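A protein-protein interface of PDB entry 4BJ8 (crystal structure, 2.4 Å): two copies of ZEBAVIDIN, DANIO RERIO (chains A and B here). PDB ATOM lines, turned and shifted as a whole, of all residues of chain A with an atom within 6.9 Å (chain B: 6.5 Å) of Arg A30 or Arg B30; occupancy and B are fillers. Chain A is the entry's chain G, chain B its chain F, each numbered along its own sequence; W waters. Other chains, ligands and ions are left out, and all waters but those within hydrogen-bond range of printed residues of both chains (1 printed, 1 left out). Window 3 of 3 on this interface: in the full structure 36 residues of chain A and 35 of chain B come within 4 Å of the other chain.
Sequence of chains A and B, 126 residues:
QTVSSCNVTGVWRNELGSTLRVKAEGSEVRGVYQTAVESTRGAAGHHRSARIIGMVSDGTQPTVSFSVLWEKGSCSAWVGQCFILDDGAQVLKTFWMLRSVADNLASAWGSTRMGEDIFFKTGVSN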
ATOM      1  N   ARG A  21      29.910   6.766  29.480  1.00  0.00           N
ATOM      2  CA  ARG A  21      30.427   5.392  29.325  1.00  0.00           C
ATOM      3  C   ARG A  21      30.033   4.811  27.987  1.00  0.00           C
ATOM      4  O   ARG A  21      28.845   4.582  27.728  1.00  0.00           O
ATOM      5  CB  ARG A  21      29.981   4.420  30.431  1.00  0.00           C
ATOM      6  CG  ARG A  21      30.667   3.042  30.258  1.00  0.00           C
ATOM      7  CD  ARG A  21      30.473   2.035  31.385  1.00  0.00           C
ATOM      8  NE  ARG A  21      29.130   1.447  31.410  1.00  0.00           N
ATOM      9  CZ  ARG A  21      28.092   1.957  32.074  1.00  0.00           C
ATOM     10  NH1 ARG A  21      28.223   3.095  32.790  1.00  0.00           N
ATOM     11  NH2 ARG A  21      26.915   1.326  32.027  1.00  0.00           N
ATOM     12  N   VAL A  22      31.055   4.560  27.165  1.00  0.00           N
ATOM     13  CA  VAL A  22      30.906   4.088  25.784  1.00  0.00           C
ATOM     14  C   VAL A  22      31.373   2.613  25.583  1.00  0.00           C
ATOM     15  O   VAL A  22      32.517   2.227  25.899  1.00  0.00           O
ATOM     16  CB  VAL A  22      31.718   4.967  24.813  1.00  0.00           C
ATOM     17  CG1 VAL A  22      31.566   4.479  23.379  1.00  0.00           C
ATOM     18  CG2 VAL A  22      31.313   6.427  24.918  1.00  0.00           C
ATOM     19  N   LYS A  23      30.468   1.844  24.984  1.00  0.00           N
ATOM     20  CA  LYS A  23      30.691   0.499  24.527  1.00  0.00           C
ATOM     21  C   LYS A  23      30.410   0.467  23.022  1.00  0.00           C
ATOM     22  O   LYS A  23      29.306   0.731  22.587  1.00  0.00           O
ATOM     23  CB  LYS A  23      29.705  -0.379  25.279  1.00  0.00           C
ATOM     24  CG  LYS A  23      29.452  -1.784  24.757  1.00  0.00           C
ATOM     25  CD  LYS A  23      28.153  -2.332  25.363  1.00  0.00           C
ATOM     26  CE  LYS A  23      28.365  -3.672  26.044  1.00  0.00           C
ATOM     27  NZ  LYS A  23      28.630  -4.754  25.064  1.00  0.00           N
ATOM     28  N   ALA A  24      31.412   0.160  22.212  1.00  0.00           N
ATOM     29  CA  ALA A  24      31.180  -0.055  20.772  1.00  0.00           C
ATOM     30  C   ALA A  24      30.651  -1.454  20.487  1.00  0.00           C
ATOM     31  O   ALA A  24      31.141  -2.458  21.009  1.00  0.00           O
ATOM     32  CB  ALA A  24      32.455   0.175  19.981  1.00  0.00           C
ATOM     33  N   GLU A  25      29.640  -1.515  19.647  1.00  0.00           N
ATOM     34  CA  GLU A  25      29.173  -2.777  19.125  1.00  0.00           C
ATOM     35  C   GLU A  25      29.017  -2.582  17.633  1.00  0.00           C
ATOM     36  O   GLU A  25      27.965  -2.125  17.133  1.00  0.00           O
ATOM     37  CB  GLU A  25      27.888  -3.243  19.787  1.00  0.00           C
ATOM     38  CG  GLU A  25      26.966  -2.169  20.300  1.00  0.00           C
ATOM     39  CD  GLU A  25      25.998  -2.743  21.312  1.00  0.00           C
ATOM     40  OE1 GLU A  25      26.437  -3.093  22.431  1.00  0.00           O
ATOM     41  OE2 GLU A  25      24.807  -2.862  20.977  1.00  0.00           O
ATOM     42  N   GLU A  28      27.996   0.837  15.909  1.00  0.00           N
ATOM     43  CA  GLU A  28      27.137   1.509  16.849  1.00  0.00           C
ATOM     44  C   GLU A  28      27.907   1.740  18.107  1.00  0.00           C
ATOM     45  O   GLU A  28      28.894   1.063  18.358  1.00  0.00           O
ATOM     46  CB  GLU A  28      25.885   0.673  17.136  1.00  0.00           C
ATOM     47  CG  GLU A  28      25.218   0.228  15.835  1.00  0.00           C
ATOM     48  CD  GLU A  28      23.803  -0.274  15.991  1.00  0.00           C
ATOM     49  OE1 GLU A  28      23.345  -0.488  17.159  1.00  0.00           O
ATOM     50  OE2 GLU A  28      23.178  -0.435  14.911  1.00  0.00           O
ATOM     51  N   VAL A  29      27.462   2.728  18.869  1.00  0.00           N
ATOM     52  CA  VAL A  29      27.888   2.913  20.243  1.00  0.00           C
ATOM     53  C   VAL A  29      26.638   2.791  21.081  1.00  0.00           C
ATOM     54  O   VAL A  29      25.545   3.197  20.649  1.00  0.00           O
ATOM     55  CB  VAL A  29      28.564   4.269  20.497  1.00  0.00           C
ATOM     56  CG1 VAL A  29      30.014   4.234  20.044  1.00  0.00           C
ATOM     57  CG2 VAL A  29      27.843   5.400  19.798  1.00  0.00           C
ATOM     58  N   ARG A  30      26.803   2.179  22.247  1.00  0.00           N
ATOM     59  CA  ARG A  30      25.784   2.120  23.282  1.00  0.00           C
ATOM     60  C   ARG A  30      26.471   2.522  24.563  1.00  0.00           C
ATOM     61  O   ARG A  30      27.664   2.816  24.518  1.00  0.00           O
ATOM     62  CB  ARG A  30      25.171   0.737  23.361  1.00  0.00           C
ATOM     63  CG  ARG A  30      24.423   0.414  22.075  1.00  0.00           C
ATOM     64  CD  ARG A  30      23.017  -0.101  22.301  1.00  0.00           C
ATOM     65  NE  ARG A  30      22.239  -0.073  21.056  1.00  0.00           N
ATOM     66  CZ  ARG A  30      20.911  -0.192  20.992  1.00  0.00           C
ATOM     67  NH1 ARG A  30      20.181  -0.345  22.098  1.00  0.00           N
ATOM     68  NH2 ARG A  30      20.298  -0.147  19.820  1.00  0.00           N
ATOM     69  N   GLY A  31      25.732   2.598  25.672  1.00  0.00           N
ATOM     70  CA  GLY A  31      26.306   3.059  26.941  1.00  0.00           C
ATOM     71  C   GLY A  31      25.425   3.962  27.812  1.00  0.00           C
ATOM     72  O   GLY A  31      24.204   4.035  27.653  1.00  0.00           O
ATOM     73  N   VAL A  32      26.071   4.664  28.737  1.00  0.00           N
ATOM     74  CA  VAL A  32      25.385   5.433  29.786  1.00  0.00           C
ATOM     75  C   VAL A  32      25.951   6.855  29.881  1.00  0.00           C
ATOM     76  O   VAL A  32      27.180   7.046  29.815  1.00  0.00           O
ATOM     77  CB  VAL A  32      25.464   4.656  31.127  1.00  0.00           C
ATOM     78  CG1 VAL A  32      24.974   5.473  32.319  1.00  0.00           C
ATOM     79  CG2 VAL A  32      24.628   3.392  31.010  1.00  0.00           C
ATOM     80  N   ARG A  51      20.504   6.502  28.644  1.00  0.00           N
ATOM     81  CA  ARG A  51      21.276   5.652  27.775  1.00  0.00           C
ATOM     82  C   ARG A  51      21.725   6.451  26.544  1.00  0.00           C
ATOM     83  O   ARG A  51      21.165   7.470  26.217  1.00  0.00           O
ATOM     84  CB  ARG A  51      20.441   4.432  27.367  1.00  0.00           C
ATOM     85  CG  ARG A  51      20.113   3.410  28.468  1.00  0.00           C
ATOM     86  CD  ARG A  51      19.783   2.077  27.799  1.00  0.00           C
ATOM     87  NE  ARG A  51      19.050   1.083  28.586  1.00  0.00           N
ATOM     88  CZ  ARG A  51      19.579  -0.001  29.177  1.00  0.00           C
ATOM     89  NH1 ARG A  51      20.896  -0.240  29.162  1.00  0.00           N
ATOM     90  NH2 ARG A  51      18.782  -0.850  29.820  1.00  0.00           N
ATOM     91  N   ILE A  52      22.720   5.910  25.857  1.00  0.00           N
ATOM     92  CA  ILE A  52      23.297   6.474  24.654  1.00  0.00           C
ATOM     93  C   ILE A  52      23.095   5.580  23.418  1.00  0.00           C
ATOM     94  O   ILE A  52      23.126   4.356  23.496  1.00  0.00           O
ATOM     95  CB  ILE A  52      24.778   6.691  24.946  1.00  0.00           C
ATOM     96  CG1 ILE A  52      24.939   7.992  25.712  1.00  0.00           C
ATOM     97  CG2 ILE A  52      25.659   6.614  23.705  1.00  0.00           C
ATOM     98  CD1 ILE A  52      26.079   7.914  26.697  1.00  0.00           C
ATOM     99  N   ILE A  53      22.873   6.214  22.275  1.00  0.00           N
ATOM    100  CA  ILE A  53      22.830   5.505  21.021  1.00  0.00           C
ATOM    101  C   ILE A  53      23.398   6.348  19.859  1.00  0.00           C
ATOM    102  O   ILE A  53      23.131   7.563  19.736  1.00  0.00           O
ATOM    103  CB  ILE A  53      21.408   5.003  20.747  1.00  0.00           C
ATOM    104  CG1 ILE A  53      21.437   3.847  19.737  1.00  0.00           C
ATOM    105  CG2 ILE A  53      20.512   6.116  20.237  1.00  0.00           C
ATOM    106  CD1 ILE A  53      20.081   3.196  19.504  1.00  0.00           C
ATOM    107  N   GLY A  54      24.191   5.692  19.015  1.00  0.00           N
ATOM    108  CA  GLY A  54      24.923   6.393  17.962  1.00  0.00           C
ATOM    109  C   GLY A  54      25.894   5.550  17.156  1.00  0.00           C
ATOM    110  O   GLY A  54      25.799   4.308  17.120  1.00  0.00           O
ATOM    111  N   ARG B  21      13.931   7.837   5.548  1.00  0.00           N
ATOM    112  CA  ARG B  21      13.074   6.692   5.852  1.00  0.00           C
ATOM    113  C   ARG B  21      13.434   6.198   7.223  1.00  0.00           C
ATOM    114  O   ARG B  21      14.568   5.804   7.473  1.00  0.00           O
ATOM    115  CB  ARG B  21      13.261   5.550   4.858  1.00  0.00           C
ATOM    116  CG  ARG B  21      13.374   6.002   3.422  1.00  0.00           C
ATOM    117  CD  ARG B  21      12.960   4.913   2.446  1.00  0.00           C
ATOM    118  NE  ARG B  21      12.883   5.439   1.084  1.00  0.00           N
ATOM    119  CZ  ARG B  21      13.936   5.720   0.317  1.00  0.00           C
ATOM    120  NH1 ARG B  21      15.176   5.536   0.756  1.00  0.00           N
ATOM    121  NH2 ARG B  21      13.745   6.191  -0.911  1.00  0.00           N
ATOM    122  N   VAL B  22      12.442   6.203   8.096  1.00  0.00           N
ATOM    123  CA  VAL B  22      12.632   5.869   9.492  1.00  0.00           C
ATOM    124  C   VAL B  22      11.494   4.943   9.917  1.00  0.00           C
ATOM    125  O   VAL B  22      10.383   5.011   9.362  1.00  0.00           O
ATOM    126  CB  VAL B  22      12.690   7.162  10.362  1.00  0.00           C
ATOM    127  CG1 VAL B  22      11.405   7.970  10.237  1.00  0.00           C
ATOM    128  CG2 VAL B  22      12.995   6.852  11.825  1.00  0.00           C
ATOM    129  N   LYS B  23      11.795   4.055  10.862  1.00  0.00           N
ATOM    130  CA  LYS B  23      10.777   3.280  11.561  1.00  0.00           C
ATOM    131  C   LYS B  23      11.128   3.375  13.032  1.00  0.00           C
ATOM    132  O   LYS B  23      12.286   3.586  13.351  1.00  0.00           O
ATOM    133  CB  LYS B  23      10.724   1.822  11.055  1.00  0.00           C
ATOM    134  CG  LYS B  23      11.838   0.897  11.551  1.00  0.00           C
ATOM    135  CD  LYS B  23      12.007  -0.331  10.641  1.00  0.00           C
ATOM    136  CE  LYS B  23      12.574  -1.561  11.354  1.00  0.00           C
ATOM    137  NZ  LYS B  23      14.017  -1.425  11.713  1.00  0.00           N
ATOM    138  N   ALA B  24      10.120   3.258  13.903  1.00  0.00           N
ATOM    139  CA  ALA B  24      10.256   3.422  15.371  1.00  0.00           C
ATOM    140  C   ALA B  24       9.924   2.133  16.122  1.00  0.00           C
ATOM    141  O   ALA B  24       8.969   1.437  15.770  1.00  0.00           O
ATOM    142  CB  ALA B  24       9.340   4.533  15.862  1.00  0.00           C
ATOM    143  N   GLU B  25      10.693   1.851  17.176  1.00  0.00           N
ATOM    144  CA  GLU B  25      10.624   0.575  17.904  1.00  0.00           C
ATOM    145  C   GLU B  25      10.935   0.764  19.389  1.00  0.00           C
ATOM    146  O   GLU B  25      12.086   0.847  19.791  1.00  0.00           O
ATOM    147  CB  GLU B  25      11.594  -0.428  17.283  1.00  0.00           C
ATOM    148  CG  GLU B  25      11.689  -1.747  18.024  1.00  0.00           C
ATOM    149  CD  GLU B  25      11.605  -2.937  17.087  1.00  0.00           C
ATOM    150  OE1 GLU B  25      10.482  -3.279  16.671  1.00  0.00           O
ATOM    151  OE2 GLU B  25      12.650  -3.524  16.748  1.00  0.00           O
ATOM    152  N   GLU B  28      13.368   3.633  20.149  1.00  0.00           N
ATOM    153  CA  GLU B  28      14.518   3.611  19.253  1.00  0.00           C
ATOM    154  C   GLU B  28      14.043   3.828  17.830  1.00  0.00           C
ATOM    155  O   GLU B  28      13.031   3.269  17.437  1.00  0.00           O
ATOM    156  CB  GLU B  28      15.316   2.315  19.432  1.00  0.00           C
ATOM    157  CG  GLU B  28      15.972   2.257  20.816  1.00  0.00           C
ATOM    158  CD  GLU B  28      17.032   1.167  21.001  1.00  0.00           C
ATOM    159  OE1 GLU B  28      17.589   0.627  20.015  1.00  0.00           O
ATOM    160  OE2 GLU B  28      17.319   0.859  22.177  1.00  0.00           O
ATOM    161  N   VAL B  29      14.733   4.712  17.104  1.00  0.00           N
ATOM    162  CA  VAL B  29      14.519   4.905  15.656  1.00  0.00           C
ATOM    163  C   VAL B  29      15.668   4.331  14.809  1.00  0.00           C
ATOM    164  O   VAL B  29      16.821   4.351  15.225  1.00  0.00           O
ATOM    165  CB  VAL B  29      14.319   6.400  15.241  1.00  0.00           C
ATOM    166  CG1 VAL B  29      13.048   6.949  15.850  1.00  0.00           C
ATOM    167  CG2 VAL B  29      15.501   7.283  15.597  1.00  0.00           C
ATOM    168  N   ARG B  30      15.323   3.836  13.621  1.00  0.00           N
ATOM    169  CA  ARG B  30      16.288   3.255  12.668  1.00  0.00           C
ATOM    170  C   ARG B  30      15.813   3.540  11.250  1.00  0.00           C
ATOM    171  O   ARG B  30      14.686   3.982  11.041  1.00  0.00           O
ATOM    172  CB  ARG B  30      16.439   1.742  12.876  1.00  0.00           C
ATOM    173  CG  ARG B  30      17.121   1.389  14.184  1.00  0.00           C
ATOM    174  CD  ARG B  30      16.955  -0.063  14.616  1.00  0.00           C
ATOM    175  NE  ARG B  30      17.798  -0.339  15.781  1.00  0.00           N
ATOM    176  CZ  ARG B  30      19.125  -0.515  15.739  1.00  0.00           C
ATOM    177  NH1 ARG B  30      19.793  -0.458  14.590  1.00  0.00           N
ATOM    178  NH2 ARG B  30      19.802  -0.747  16.859  1.00  0.00           N
ATOM    179  N   GLY B  31      16.667   3.328  10.265  1.00  0.00           N
ATOM    180  CA  GLY B  31      16.256   3.609   8.899  1.00  0.00           C
ATOM    181  C   GLY B  31      17.375   4.116   8.059  1.00  0.00           C
ATOM    182  O   GLY B  31      18.508   3.877   8.392  1.00  0.00           O
ATOM    183  N   VAL B  32      17.039   4.820   6.976  1.00  0.00           N
ATOM    184  CA  VAL B  32      18.005   5.255   5.963  1.00  0.00           C
ATOM    185  C   VAL B  32      17.761   6.728   5.688  1.00  0.00           C
ATOM    186  O   VAL B  32      16.619   7.188   5.691  1.00  0.00           O
ATOM    187  CB  VAL B  32      17.872   4.466   4.628  1.00  0.00           C
ATOM    188  CG1 VAL B  32      19.019   4.795   3.675  1.00  0.00           C
ATOM    189  CG2 VAL B  32      17.843   2.960   4.883  1.00  0.00           C
ATOM    190  N   ARG B  51      22.714   4.723   7.003  1.00  0.00           N
ATOM    191  CA  ARG B  51      21.737   4.343   7.992  1.00  0.00           C
ATOM    192  C   ARG B  51      21.637   5.405   9.059  1.00  0.00           C
ATOM    193  O   ARG B  51      22.570   6.204   9.261  1.00  0.00           O
ATOM    194  CB  ARG B  51      22.080   3.016   8.639  1.00  0.00           C
ATOM    195  CG  ARG B  51      21.960   1.826   7.693  1.00  0.00           C
ATOM    196  CD  ARG B  51      20.994   0.768   8.218  1.00  0.00           C
ATOM    197  NE  ARG B  51      21.355  -0.567   7.746  1.00  0.00           N
ATOM    198  CZ  ARG B  51      22.308  -1.327   8.292  1.00  0.00           C
ATOM    199  NH1 ARG B  51      23.013  -0.890   9.340  1.00  0.00           N
ATOM    200  NH2 ARG B  51      22.567  -2.533   7.782  1.00  0.00           N
ATOM    201  N   ILE B  52      20.488   5.416   9.729  1.00  0.00           N
ATOM    202  CA  ILE B  52      20.245   6.332  10.820  1.00  0.00           C
ATOM    203  C   ILE B  52      20.052   5.526  12.100  1.00  0.00           C
ATOM    204  O   ILE B  52      19.518   4.412  12.074  1.00  0.00           O
ATOM    205  CB  ILE B  52      19.020   7.250  10.537  1.00  0.00           C
ATOM    206  CG1 ILE B  52      17.697   6.572  10.905  1.00  0.00           C
ATOM    207  CG2 ILE B  52      18.986   7.684   9.079  1.00  0.00           C
ATOM    208  CD1 ILE B  52      16.479   7.446  10.683  1.00  0.00           C
ATOM    209  N   ILE B  53      20.499   6.077  13.219  1.00  0.00           N
ATOM    210  CA  ILE B  53      20.186   5.494  14.526  1.00  0.00           C
ATOM    211  C   ILE B  53      19.906   6.609  15.517  1.00  0.00           C
ATOM    212  O   ILE B  53      20.499   7.666  15.433  1.00  0.00           O
ATOM    213  CB  ILE B  53      21.288   4.570  15.008  1.00  0.00           C
ATOM    214  CG1 ILE B  53      20.769   3.694  16.138  1.00  0.00           C
ATOM    215  CG2 ILE B  53      22.507   5.352  15.455  1.00  0.00           C
ATOM    216  CD1 ILE B  53      21.734   2.592  16.544  1.00  0.00           C
ATOM    217  N   GLY B  54      18.967   6.389  16.422  1.00  0.00           N
ATOM    218  CA  GLY B  54      18.551   7.440  17.337  1.00  0.00           C
ATOM    219  C   GLY B  54      17.386   7.095  18.254  1.00  0.00           C
ATOM    220  O   GLY B  54      17.136   5.936  18.551  1.00  0.00           O
HETATM  221  O   HOH W   1      23.927   0.659  12.093  1.00  0.00           O
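Arg A30 touches just these residues of chain B: Glu B28 and Arg B30.
Arg B30 touches just these residues of chain A: Glu A28 and Arg A30.
Printed residues of chain A within 4 Å of Glu B28: Arg A30 (2.8 Å) and Ile A53 (3.6 Å).
Printed residues of chain B within 4 Å of Glu A28: Arg B30 (3.4 Å) and Ile B53 (3.5 Å).
The nearest printed residue of chain B that does not touch Glu A28 is Arg B51 (5.6 Å).
The side-chain carboxylate of Glu B28 is in salt-bridge range of the guanidinium group of Arg A30 (2.8 Å).
The side-chain carboxylate (OE2) of Glu A28 is in salt-bridge range of the guanidinium group (NH1) of Arg B30 (3.4 Å).
The guanidinium group of Arg B30 sits close to the guanidinium group of Arg A30, at 3.1 Å.
Glu A28 touches Arg B30, and with the chains exchanged Arg A30 touches Glu B28.
Arg A30 touches its own counterpart, Arg B30.
Ile B53 touches its own counterpart, Ile A53.
Ile A53 touches Gly B54, and with the chains exchanged Gly A54 touches Ile B53.
Of the 8 pairs that touch across the chains among the printed residues, 8 have their exchanged pair printed and touching as well.
Water W1 lies within hydrogen-bond range of the side-chain carboxylate (OE2) of Glu A28 and the guanidinium group (NH1) of Arg B51.
N of Lys B23 lies within hydrogen-bond range of O of Arg B30.
N of Val B29 lies within hydrogen-bond range of O of Gly B54 (3.1 Å).
N of Arg A30 sits at hydrogen-bond distance from O of Lys A23, 2.9 Å away.
The side-chain carboxylate (OE2) of Glu A25 lies within salt-bridge range of the guanidinium group (NE) of Arg A30.
O of Gly A54 lies within hydrogen-bond range of N of Val A29, at 2.9 Å.
Printed residues of chain A that touch a printed residue of chain B: Glu A28, Arg A30, Ile A53 and Gly A54.
Among the printed residues, Asp or Glu carboxylates within 4 Å of a Lys or Arg side-chain nitrogen of the other chain: Glu A28 with Arg B30 (3.4 Å) and Arg A30 with Glu B28 (2.8 Å).
Ile B53 touches Glu A28 (CD1 to OE1, 3.5 Å).
Glu B28 touches Ile A53 (OE1 to CD1, 3.6 Å).
Ile B53 touches Ile A53 (CD1 to CG1, 3.4 Å).
CG2 of Ile A53 touches CA of Gly B54, 3.7 Å away.
Gly A54 touches Ile B53 (CA to CG2, 3.6 Å).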
